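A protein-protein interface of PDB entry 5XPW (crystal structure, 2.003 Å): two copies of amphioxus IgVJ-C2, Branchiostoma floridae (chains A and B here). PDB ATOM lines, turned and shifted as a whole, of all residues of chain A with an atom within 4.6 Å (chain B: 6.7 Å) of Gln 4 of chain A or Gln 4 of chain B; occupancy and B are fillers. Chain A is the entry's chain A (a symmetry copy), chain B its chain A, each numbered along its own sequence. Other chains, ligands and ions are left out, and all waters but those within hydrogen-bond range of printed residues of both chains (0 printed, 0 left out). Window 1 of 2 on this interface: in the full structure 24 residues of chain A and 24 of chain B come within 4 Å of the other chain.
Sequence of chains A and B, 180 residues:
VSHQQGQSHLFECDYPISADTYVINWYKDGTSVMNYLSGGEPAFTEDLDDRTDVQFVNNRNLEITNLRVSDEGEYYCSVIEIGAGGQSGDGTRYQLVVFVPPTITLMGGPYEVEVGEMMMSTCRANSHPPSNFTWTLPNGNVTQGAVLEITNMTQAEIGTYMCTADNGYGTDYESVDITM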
ATOM      1  N   HIS A   3       8.993  -8.584 -21.615  1.00  0.00           N
ATOM      2  CA  HIS A   3      10.365  -8.109 -21.723  1.00  0.00           C
ATOM      3  C   HIS A   3      10.511  -6.885 -20.835  1.00  0.00           C
ATOM      4  O   HIS A   3       9.515  -6.294 -20.425  1.00  0.00           O
ATOM      5  CB  HIS A   3      10.682  -7.711 -23.169  1.00  0.00           C
ATOM      6  CG  HIS A   3      10.677  -8.861 -24.126  1.00  0.00           C
ATOM      7  ND1 HIS A   3       9.619  -9.121 -24.973  1.00  0.00           N
ATOM      8  CD2 HIS A   3      11.595  -9.823 -24.371  1.00  0.00           C
ATOM      9  CE1 HIS A   3       9.890 -10.192 -25.697  1.00  0.00           C
ATOM     10  NE2 HIS A   3      11.087 -10.636 -25.351  1.00  0.00           N
ATOM     11  N   GLN A   4      11.749  -6.496 -20.552  1.00  0.00           N
ATOM     12  CA  GLN A   4      12.005  -5.237 -19.870  1.00  0.00           C
ATOM     13  C   GLN A   4      12.258  -4.160 -20.905  1.00  0.00           C
ATOM     14  O   GLN A   4      12.506  -4.463 -22.070  1.00  0.00           O
ATOM     15  CB  GLN A   4      13.205  -5.350 -18.925  1.00  0.00           C
ATOM     16  CG  GLN A   4      12.989  -6.291 -17.759  1.00  0.00           C
ATOM     17  CD  GLN A   4      13.896  -5.979 -16.578  1.00  0.00           C
ATOM     18  OE1 GLN A   4      14.331  -6.879 -15.862  1.00  0.00           O
ATOM     19  NE2 GLN A   4      14.181  -4.697 -16.369  1.00  0.00           N
ATOM     20  N   GLN A   5      12.184  -2.901 -20.477  1.00  0.00           N
ATOM     21  CA  GLN A   5      12.409  -1.774 -21.375  1.00  0.00           C
ATOM     22  C   GLN A   5      13.793  -1.850 -22.020  1.00  0.00           C
ATOM     23  O   GLN A   5      14.766  -2.247 -21.382  1.00  0.00           O
ATOM     24  CB  GLN A   5      12.243  -0.448 -20.629  1.00  0.00           C
ATOM     25  CG  GLN A   5      10.813  -0.161 -20.181  1.00  0.00           C
ATOM     26  CD  GLN A   5      10.587   1.303 -19.825  1.00  0.00           C
ATOM     27  OE1 GLN A   5      11.140   1.812 -18.848  1.00  0.00           O
ATOM     28  NE2 GLN A   5       9.764   1.985 -20.618  1.00  0.00           N
ATOM     29  N   GLY A   6      13.870  -1.484 -23.295  1.00  0.00           N
ATOM     30  CA  GLY A   6      15.140  -1.455 -23.999  1.00  0.00           C
ATOM     31  C   GLY A   6      15.432  -2.747 -24.737  1.00  0.00           C
ATOM     32  O   GLY A   6      16.286  -2.795 -25.626  1.00  0.00           O
ATOM     33  N   GLN A   7      14.724  -3.806 -24.364  1.00  0.00           N
ATOM     34  CA  GLN A   7      14.882  -5.087 -25.034  1.00  0.00           C
ATOM     35  C   GLN A   7      14.075  -5.112 -26.333  1.00  0.00           C
ATOM     36  O   GLN A   7      13.303  -4.187 -26.606  1.00  0.00           O
ATOM     37  CB  GLN A   7      14.501  -6.232 -24.089  1.00  0.00           C
ATOM     38  CG  GLN A   7      15.450  -6.331 -22.875  1.00  0.00           C
ATOM     39  CD  GLN A   7      15.141  -7.504 -21.960  1.00  0.00           C
ATOM     40  OE1 GLN A   7      13.989  -7.915 -21.819  1.00  0.00           O
ATOM     41  NE2 GLN A   7      16.175  -8.050 -21.337  1.00  0.00           N
ATOM     42  N   LEU A  67      12.030  -1.503 -26.668  1.00  0.00           N
ATOM     43  CA  LEU A  67      10.690  -1.550 -26.091  1.00  0.00           C
ATOM     44  C   LEU A  67      10.446  -0.483 -25.032  1.00  0.00           C
ATOM     45  O   LEU A  67      11.309  -0.203 -24.197  1.00  0.00           O
ATOM     46  CB  LEU A  67      10.397  -2.935 -25.506  1.00  0.00           C
ATOM     47  CG  LEU A  67      10.163  -4.062 -26.505  1.00  0.00           C
ATOM     48  CD1 LEU A  67      10.180  -5.408 -25.797  1.00  0.00           C
ATOM     49  CD2 LEU A  67       8.838  -3.857 -27.278  1.00  0.00           C
ATOM     50  N   VAL A  98       5.506  -5.190 -21.291  1.00  0.00           N
ATOM     51  CA  VAL A  98       6.804  -4.568 -21.034  1.00  0.00           C
ATOM     52  C   VAL A  98       6.855  -4.137 -19.575  1.00  0.00           C
ATOM     53  O   VAL A  98       6.263  -3.129 -19.199  1.00  0.00           O
ATOM     54  CB  VAL A  98       7.047  -3.343 -21.935  1.00  0.00           C
ATOM     55  CG1 VAL A  98       8.433  -2.749 -21.664  1.00  0.00           C
ATOM     56  CG2 VAL A  98       6.905  -3.725 -23.394  1.00  0.00           C
ATOM     57  N   PHE A  99       7.555  -4.910 -18.752  1.00  0.00           N
ATOM     58  CA  PHE A  99       7.542  -4.673 -17.313  1.00  0.00           C
ATOM     59  C   PHE A  99       8.750  -3.890 -16.799  1.00  0.00           C
ATOM     60  O   PHE A  99       9.827  -3.897 -17.402  1.00  0.00           O
ATOM     61  CB  PHE A  99       7.383  -5.994 -16.542  1.00  0.00           C
ATOM     62  CG  PHE A  99       8.583  -6.904 -16.621  1.00  0.00           C
ATOM     63  CD1 PHE A  99       8.717  -7.815 -17.658  1.00  0.00           C
ATOM     64  CD2 PHE A  99       9.564  -6.860 -15.643  1.00  0.00           C
ATOM     65  CE1 PHE A  99       9.816  -8.661 -17.726  1.00  0.00           C
ATOM     66  CE2 PHE A  99      10.672  -7.703 -15.704  1.00  0.00           C
ATOM     67  CZ  PHE A  99      10.797  -8.603 -16.744  1.00  0.00           C
ATOM     68  N   PRO A 101      10.589  -3.623 -12.996  1.00  0.00           N
ATOM     69  CA  PRO A 101      10.618  -4.098 -11.607  1.00  0.00           C
ATOM     70  C   PRO A 101      10.522  -2.918 -10.647  1.00  0.00           C
ATOM     71  O   PRO A 101      10.942  -1.817 -10.995  1.00  0.00           O
ATOM     72  CB  PRO A 101      11.995  -4.763 -11.492  1.00  0.00           C
ATOM     73  CG  PRO A 101      12.393  -5.077 -12.905  1.00  0.00           C
ATOM     74  CD  PRO A 101      11.822  -3.963 -13.724  1.00  0.00           C
ATOM     75  N   SER B   2      21.167 -11.046  -5.085  1.00  0.00           N
ATOM     76  CA  SER B   2      21.109 -10.178  -6.256  1.00  0.00           C
ATOM     77  C   SER B   2      19.912  -9.234  -6.299  1.00  0.00           C
ATOM     78  O   SER B   2      18.824  -9.559  -5.831  1.00  0.00           O
ATOM     79  CB  SER B   2      21.169 -11.010  -7.537  1.00  0.00           C
ATOM     80  OG  SER B   2      20.151 -11.988  -7.548  1.00  0.00           O
ATOM     81  N   HIS B   3      20.142  -8.059  -6.874  1.00  0.00           N
ATOM     82  CA  HIS B   3      19.106  -7.056  -7.073  1.00  0.00           C
ATOM     83  C   HIS B   3      19.405  -6.319  -8.367  1.00  0.00           C
ATOM     84  O   HIS B   3      20.517  -6.400  -8.883  1.00  0.00           O
ATOM     85  CB  HIS B   3      19.109  -6.048  -5.918  1.00  0.00           C
ATOM     86  CG  HIS B   3      18.718  -6.638  -4.601  1.00  0.00           C
ATOM     87  ND1 HIS B   3      19.641  -6.971  -3.630  1.00  0.00           N
ATOM     88  CD2 HIS B   3      17.508  -6.960  -4.089  1.00  0.00           C
ATOM     89  CE1 HIS B   3      19.014  -7.471  -2.581  1.00  0.00           C
ATOM     90  NE2 HIS B   3      17.716  -7.472  -2.834  1.00  0.00           N
ATOM     91  N   GLN B   4      18.421  -5.592  -8.882  1.00  0.00           N
ATOM     92  CA  GLN B   4      18.652  -4.702 -10.009  1.00  0.00           C
ATOM     93  C   GLN B   4      18.960  -3.314  -9.485  1.00  0.00           C
ATOM     94  O   GLN B   4      18.709  -3.020  -8.318  1.00  0.00           O
ATOM     95  CB  GLN B   4      17.437  -4.655 -10.940  1.00  0.00           C
ATOM     96  CG  GLN B   4      17.142  -5.966 -11.640  1.00  0.00           C
ATOM     97  CD  GLN B   4      16.348  -5.778 -12.923  1.00  0.00           C
ATOM     98  OE1 GLN B   4      15.520  -6.614 -13.280  1.00  0.00           O
ATOM     99  NE2 GLN B   4      16.605  -4.678 -13.627  1.00  0.00           N
ATOM    100  N   GLN B   5      19.512  -2.466 -10.350  1.00  0.00           N
ATOM    101  CA  GLN B   5      19.852  -1.100  -9.969  1.00  0.00           C
ATOM    102  C   GLN B   5      18.623  -0.344  -9.465  1.00  0.00           C
ATOM    103  O   GLN B   5      17.522  -0.510  -9.986  1.00  0.00           O
ATOM    104  CB  GLN B   5      20.489  -0.354 -11.145  1.00  0.00           C
ATOM    105  CG  GLN B   5      21.865  -0.879 -11.543  1.00  0.00           C
ATOM    106  CD  GLN B   5      22.647   0.103 -12.407  1.00  0.00           C
ATOM    107  OE1 GLN B   5      22.273   0.382 -13.547  1.00  0.00           O
ATOM    108  NE2 GLN B   5      23.744   0.625 -11.864  1.00  0.00           N
ATOM    109  N   GLY B   6      18.815   0.475  -8.435  1.00  0.00           N
ATOM    110  CA  GLY B   6      17.737   1.292  -7.907  1.00  0.00           C
ATOM    111  C   GLY B   6      17.001   0.624  -6.763  1.00  0.00           C
ATOM    112  O   GLY B   6      16.284   1.275  -5.999  1.00  0.00           O
ATOM    113  N   GLN B   7      17.171  -0.687  -6.644  1.00  0.00           N
ATOM    114  CA  GLN B   7      16.553  -1.427  -5.554  1.00  0.00           C
ATOM    115  C   GLN B   7      17.386  -1.291  -4.280  1.00  0.00           C
ATOM    116  O   GLN B   7      18.492  -0.743  -4.311  1.00  0.00           O
ATOM    117  CB  GLN B   7      16.341  -2.891  -5.960  1.00  0.00           C
ATOM    118  CG  GLN B   7      15.336  -3.039  -7.122  1.00  0.00           C
ATOM    119  CD  GLN B   7      15.051  -4.484  -7.494  1.00  0.00           C
ATOM    120  OE1 GLN B   7      15.913  -5.355  -7.370  1.00  0.00           O
ATOM    121  NE2 GLN B   7      13.835  -4.743  -7.950  1.00  0.00           N
ATOM    122  N   SER B   8      16.848  -1.754  -3.156  1.00  0.00           N
ATOM    123  CA  SER B   8      17.563  -1.675  -1.881  1.00  0.00           C
ATOM    124  C   SER B   8      18.160  -3.021  -1.497  1.00  0.00           C
ATOM    125  O   SER B   8      17.722  -4.064  -1.985  1.00  0.00           O
ATOM    126  CB  SER B   8      16.614  -1.246  -0.757  1.00  0.00           C
ATOM    127  OG  SER B   8      15.822  -0.130  -1.125  1.00  0.00           O
ATOM    128  N   ASN B  66      19.567   2.699  -3.030  1.00  0.00           N
ATOM    129  CA  ASN B  66      19.627   2.989  -4.459  1.00  0.00           C
ATOM    130  C   ASN B  66      20.849   2.295  -5.051  1.00  0.00           C
ATOM    131  O   ASN B  66      21.847   2.935  -5.386  1.00  0.00           O
ATOM    132  CB  ASN B  66      19.664   4.505  -4.704  1.00  0.00           C
ATOM    133  CG  ASN B  66      19.387   4.881  -6.163  1.00  0.00           C
ATOM    134  OD1 ASN B  66      19.250   6.062  -6.494  1.00  0.00           O
ATOM    135  ND2 ASN B  66      19.304   3.879  -7.033  1.00  0.00           N
ATOM    136  N   LEU B  67      20.764   0.973  -5.162  1.00  0.00           N
ATOM    137  CA  LEU B  67      21.909   0.159  -5.560  1.00  0.00           C
ATOM    138  C   LEU B  67      22.481   0.540  -6.919  1.00  0.00           C
ATOM    139  O   LEU B  67      21.744   0.812  -7.870  1.00  0.00           O
ATOM    140  CB  LEU B  67      21.549  -1.330  -5.550  1.00  0.00           C
ATOM    141  CG  LEU B  67      21.379  -1.980  -4.183  1.00  0.00           C
ATOM    142  CD1 LEU B  67      20.744  -3.355  -4.325  1.00  0.00           C
ATOM    143  CD2 LEU B  67      22.731  -2.067  -3.433  1.00  0.00           C
ATOM    144  N   ARG B  68      23.808   0.547  -6.989  1.00  0.00           N
ATOM    145  CA  ARG B  68      24.533   0.765  -8.228  1.00  0.00           C
ATOM    146  C   ARG B  68      25.346  -0.481  -8.497  1.00  0.00           C
ATOM    147  O   ARG B  68      25.639  -1.248  -7.576  1.00  0.00           O
ATOM    148  CB  ARG B  68      25.505   1.933  -8.084  1.00  0.00           C
ATOM    149  CG  ARG B  68      24.929   3.180  -7.461  1.00  0.00           C
ATOM    150  CD  ARG B  68      26.022   4.222  -7.288  1.00  0.00           C
ATOM    151  NE  ARG B  68      25.484   5.483  -6.795  1.00  0.00           N
ATOM    152  CZ  ARG B  68      26.197   6.594  -6.655  1.00  0.00           C
ATOM    153  NH1 ARG B  68      27.486   6.604  -6.978  1.00  0.00           N
ATOM    154  NH2 ARG B  68      25.619   7.697  -6.198  1.00  0.00           N
ATOM    155  N   VAL B  97      25.301  -8.897  -5.481  1.00  0.00           N
ATOM    156  CA  VAL B  97      25.317  -8.816  -6.932  1.00  0.00           C
ATOM    157  C   VAL B  97      24.266  -7.809  -7.372  1.00  0.00           C
ATOM    158  O   VAL B  97      23.103  -7.916  -6.990  1.00  0.00           O
ATOM    159  CB  VAL B  97      25.007 -10.188  -7.569  1.00  0.00           C
ATOM    160  CG1 VAL B  97      24.682 -10.035  -9.055  1.00  0.00           C
ATOM    161  CG2 VAL B  97      26.174 -11.156  -7.353  1.00  0.00           C
ATOM    162  N   VAL B  98      24.680  -6.821  -8.158  1.00  0.00           N
ATOM    163  CA  VAL B  98      23.742  -5.866  -8.743  1.00  0.00           C
ATOM    164  C   VAL B  98      23.748  -6.040 -10.255  1.00  0.00           C
ATOM    165  O   VAL B  98      24.670  -5.595 -10.932  1.00  0.00           O
ATOM    166  CB  VAL B  98      24.107  -4.411  -8.397  1.00  0.00           C
ATOM    167  CG1 VAL B  98      23.074  -3.446  -8.991  1.00  0.00           C
ATOM    168  CG2 VAL B  98      24.203  -4.232  -6.896  1.00  0.00           C
ATOM    169  N   PHE B  99      22.723  -6.702 -10.780  1.00  0.00           N
ATOM    170  CA  PHE B  99      22.709  -7.056 -12.195  1.00  0.00           C
ATOM    171  C   PHE B  99      21.895  -6.102 -13.069  1.00  0.00           C
ATOM    172  O   PHE B  99      20.968  -5.432 -12.603  1.00  0.00           O
ATOM    173  CB  PHE B  99      22.238  -8.507 -12.392  1.00  0.00           C
ATOM    174  CG  PHE B  99      20.781  -8.732 -12.077  1.00  0.00           C
ATOM    175  CD1 PHE B  99      20.371  -9.037 -10.788  1.00  0.00           C
ATOM    176  CD2 PHE B  99      19.826  -8.659 -13.079  1.00  0.00           C
ATOM    177  CE1 PHE B  99      19.030  -9.255 -10.500  1.00  0.00           C
ATOM    178  CE2 PHE B  99      18.479  -8.873 -12.800  1.00  0.00           C
ATOM    179  CZ  PHE B  99      18.082  -9.171 -11.510  1.00  0.00           C
ATOM    180  N   VAL B 100      22.277  -6.042 -14.340  1.00  0.00           N
ATOM    181  CA  VAL B 100      21.525  -5.329 -15.360  1.00  0.00           C
ATOM    182  C   VAL B 100      21.288  -6.308 -16.500  1.00  0.00           C
ATOM    183  O   VAL B 100      22.244  -6.860 -17.052  1.00  0.00           O
ATOM    184  CB  VAL B 100      22.299  -4.105 -15.906  1.00  0.00           C
ATOM    185  CG1 VAL B 100      21.449  -3.342 -16.912  1.00  0.00           C
ATOM    186  CG2 VAL B 100      22.745  -3.183 -14.767  1.00  0.00           C
ATOM    187  N   PRO B 101      20.014  -6.558 -16.833  1.00  0.00           N
ATOM    188  CA  PRO B 101      19.671  -7.466 -17.935  1.00  0.00           C
ATOM    189  C   PRO B 101      20.164  -6.893 -19.259  1.00  0.00           C
ATOM    190  O   PRO B 101      20.271  -5.677 -19.391  1.00  0.00           O
ATOM    191  CB  PRO B 101      18.138  -7.488 -17.908  1.00  0.00           C
ATOM    192  CG  PRO B 101      17.768  -7.047 -16.521  1.00  0.00           C
ATOM    193  CD  PRO B 101      18.818  -6.052 -16.139  1.00  0.00           C
ATOM    194  N   THR B 103      20.520  -5.401 -22.887  1.00  0.00           N
ATOM    195  CA  THR B 103      19.811  -4.709 -23.958  1.00  0.00           C
ATOM    196  C   THR B 103      20.771  -4.533 -25.127  1.00  0.00           C
ATOM    197  O   THR B 103      21.816  -3.901 -24.995  1.00  0.00           O
ATOM    198  CB  THR B 103      19.258  -3.345 -23.513  1.00  0.00           C
ATOM    199  OG1 THR B 103      20.281  -2.611 -22.826  1.00  0.00           O
ATOM    200  CG2 THR B 103      18.067  -3.534 -22.582  1.00  0.00           C
ATOM    201  N   TYR B 169      21.427 -13.375 -16.220  1.00  0.00           N
ATOM    202  CA  TYR B 169      20.429 -12.573 -15.517  1.00  0.00           C
ATOM    203  C   TYR B 169      19.412 -11.964 -16.477  1.00  0.00           C
ATOM    204  O   TYR B 169      18.869 -10.885 -16.226  1.00  0.00           O
ATOM    205  CB  TYR B 169      21.115 -11.467 -14.715  1.00  0.00           C
ATOM    206  CG  TYR B 169      21.993 -11.988 -13.596  1.00  0.00           C
ATOM    207  CD1 TYR B 169      21.471 -12.249 -12.334  1.00  0.00           C
ATOM    208  CD2 TYR B 169      23.341 -12.226 -13.805  1.00  0.00           C
ATOM    209  CE1 TYR B 169      22.276 -12.725 -11.309  1.00  0.00           C
ATOM    210  CE2 TYR B 169      24.149 -12.698 -12.790  1.00  0.00           C
ATOM    211  CZ  TYR B 169      23.613 -12.949 -11.547  1.00  0.00           C
ATOM    212  OH  TYR B 169      24.433 -13.424 -10.546  1.00  0.00           O
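Gln 4 of chain A touches two residues of chain B. Of chain A, only Gln 4 and Pro 101 come within 4 Å of Gln 4 of chain B. Printed residues of chain B within 4 Å of Gln 7 of chain A: Pro 101 (3.99 Å) and Thr 103 (3.8 Å). Printed residues of chain A within 4 Å of Pro 101 of chain B: Gln 4 (3.5 Å) and Gln 7 (3.99 Å). Val 100 of chain B touches none of the printed residues of chain A. Gly 6 of chain B touches none of the printed residues of chain A. The nearest residue of chain B that does not touch Gln 4 of chain A is Phe 99 of chain B (5.5 Å). The nearest printed residue of chain A that does not touch Gln 4 of chain B is Phe 99 of chain A (5.5 Å).
The side-chain amide oxygen (OE1) of Gln 4 of chain B lies close to the side-chain amide oxygen (OE1) of Gln 4 of chain A (2.9 Å).
Gln 4 of chain A touches its own counterpart, Gln 4 of chain B. Gln 4 of chain A touches Pro 101 of chain B, and with the chains exchanged Pro 101 of chain A touches Gln 4 of chain B. Gln 7 of chain A touches Pro 101 of chain B, and with the chains exchanged Pro 101 of chain A touches Gln 7 of chain B. Of the 8 pairs that touch across the chains among the printed residues, 5 have their exchanged pair printed and touching as well.
The backbone NH (N) of Gln 4 of chain B sits at hydrogen-bond distance from the side-chain amide oxygen (OE1) of Gln 7 of chain B (2.9 Å). The backbone NH of Leu 67 of chain B sits at hydrogen-bond distance from the backbone carbonyl oxygen of Gln 7 of chain B, at 3.0 Å. The backbone NH (N) of Gln 4 of chain A lies within hydrogen-bond range of the side-chain amide oxygen (OE1) of Gln 7 of chain A (2.9 Å). The backbone NH (N) of Gly 6 of chain A sits at hydrogen-bond distance from the backbone carbonyl oxygen (O) of Leu 67 of chain A. N of Leu 67 of chain A is in hydrogen-bond range of O of Gln 7 of chain A (3.0 Å).
Among the printed residues, pairs that only touch across the chains: Gly 6 of chain A with Thr 103 of chain B, Gln 4 of chain A with Pro 101 of chain B, Pro 101 of chain A with Gln 4 of chain B, Gln 5 of chain A with Thr 103 of chain B, Gln 7 of chain A with Thr 103 of chain B, Gln 7 of chain A with Pro 101 of chain B and Pro 101 of chain A with Gln 7 of chain B.
Of the 17 printed residues of chain B, 4 touch a printed residue of chain A. Printed residues of chain B that touch a printed residue of chain A: Gln 4, Gln 7, Pro 101 and Thr 103. Hydrophobic or aromatic side chains of chain B within 4 Å of the printed part of chain A: Pro 101. Printed residues of chain A that touch a printed residue of chain B: Gln 4, Gln 5, Gly 6, Gln 7 and Pro 101. Hydrophobic or aromatic side chains of chain A within 4 Å of the printed part of chain B: Pro 101. Among the printed residues, no Asp or Glu carboxylate lies within 4 Å of a Lys or Arg side-chain nitrogen of the other chain.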
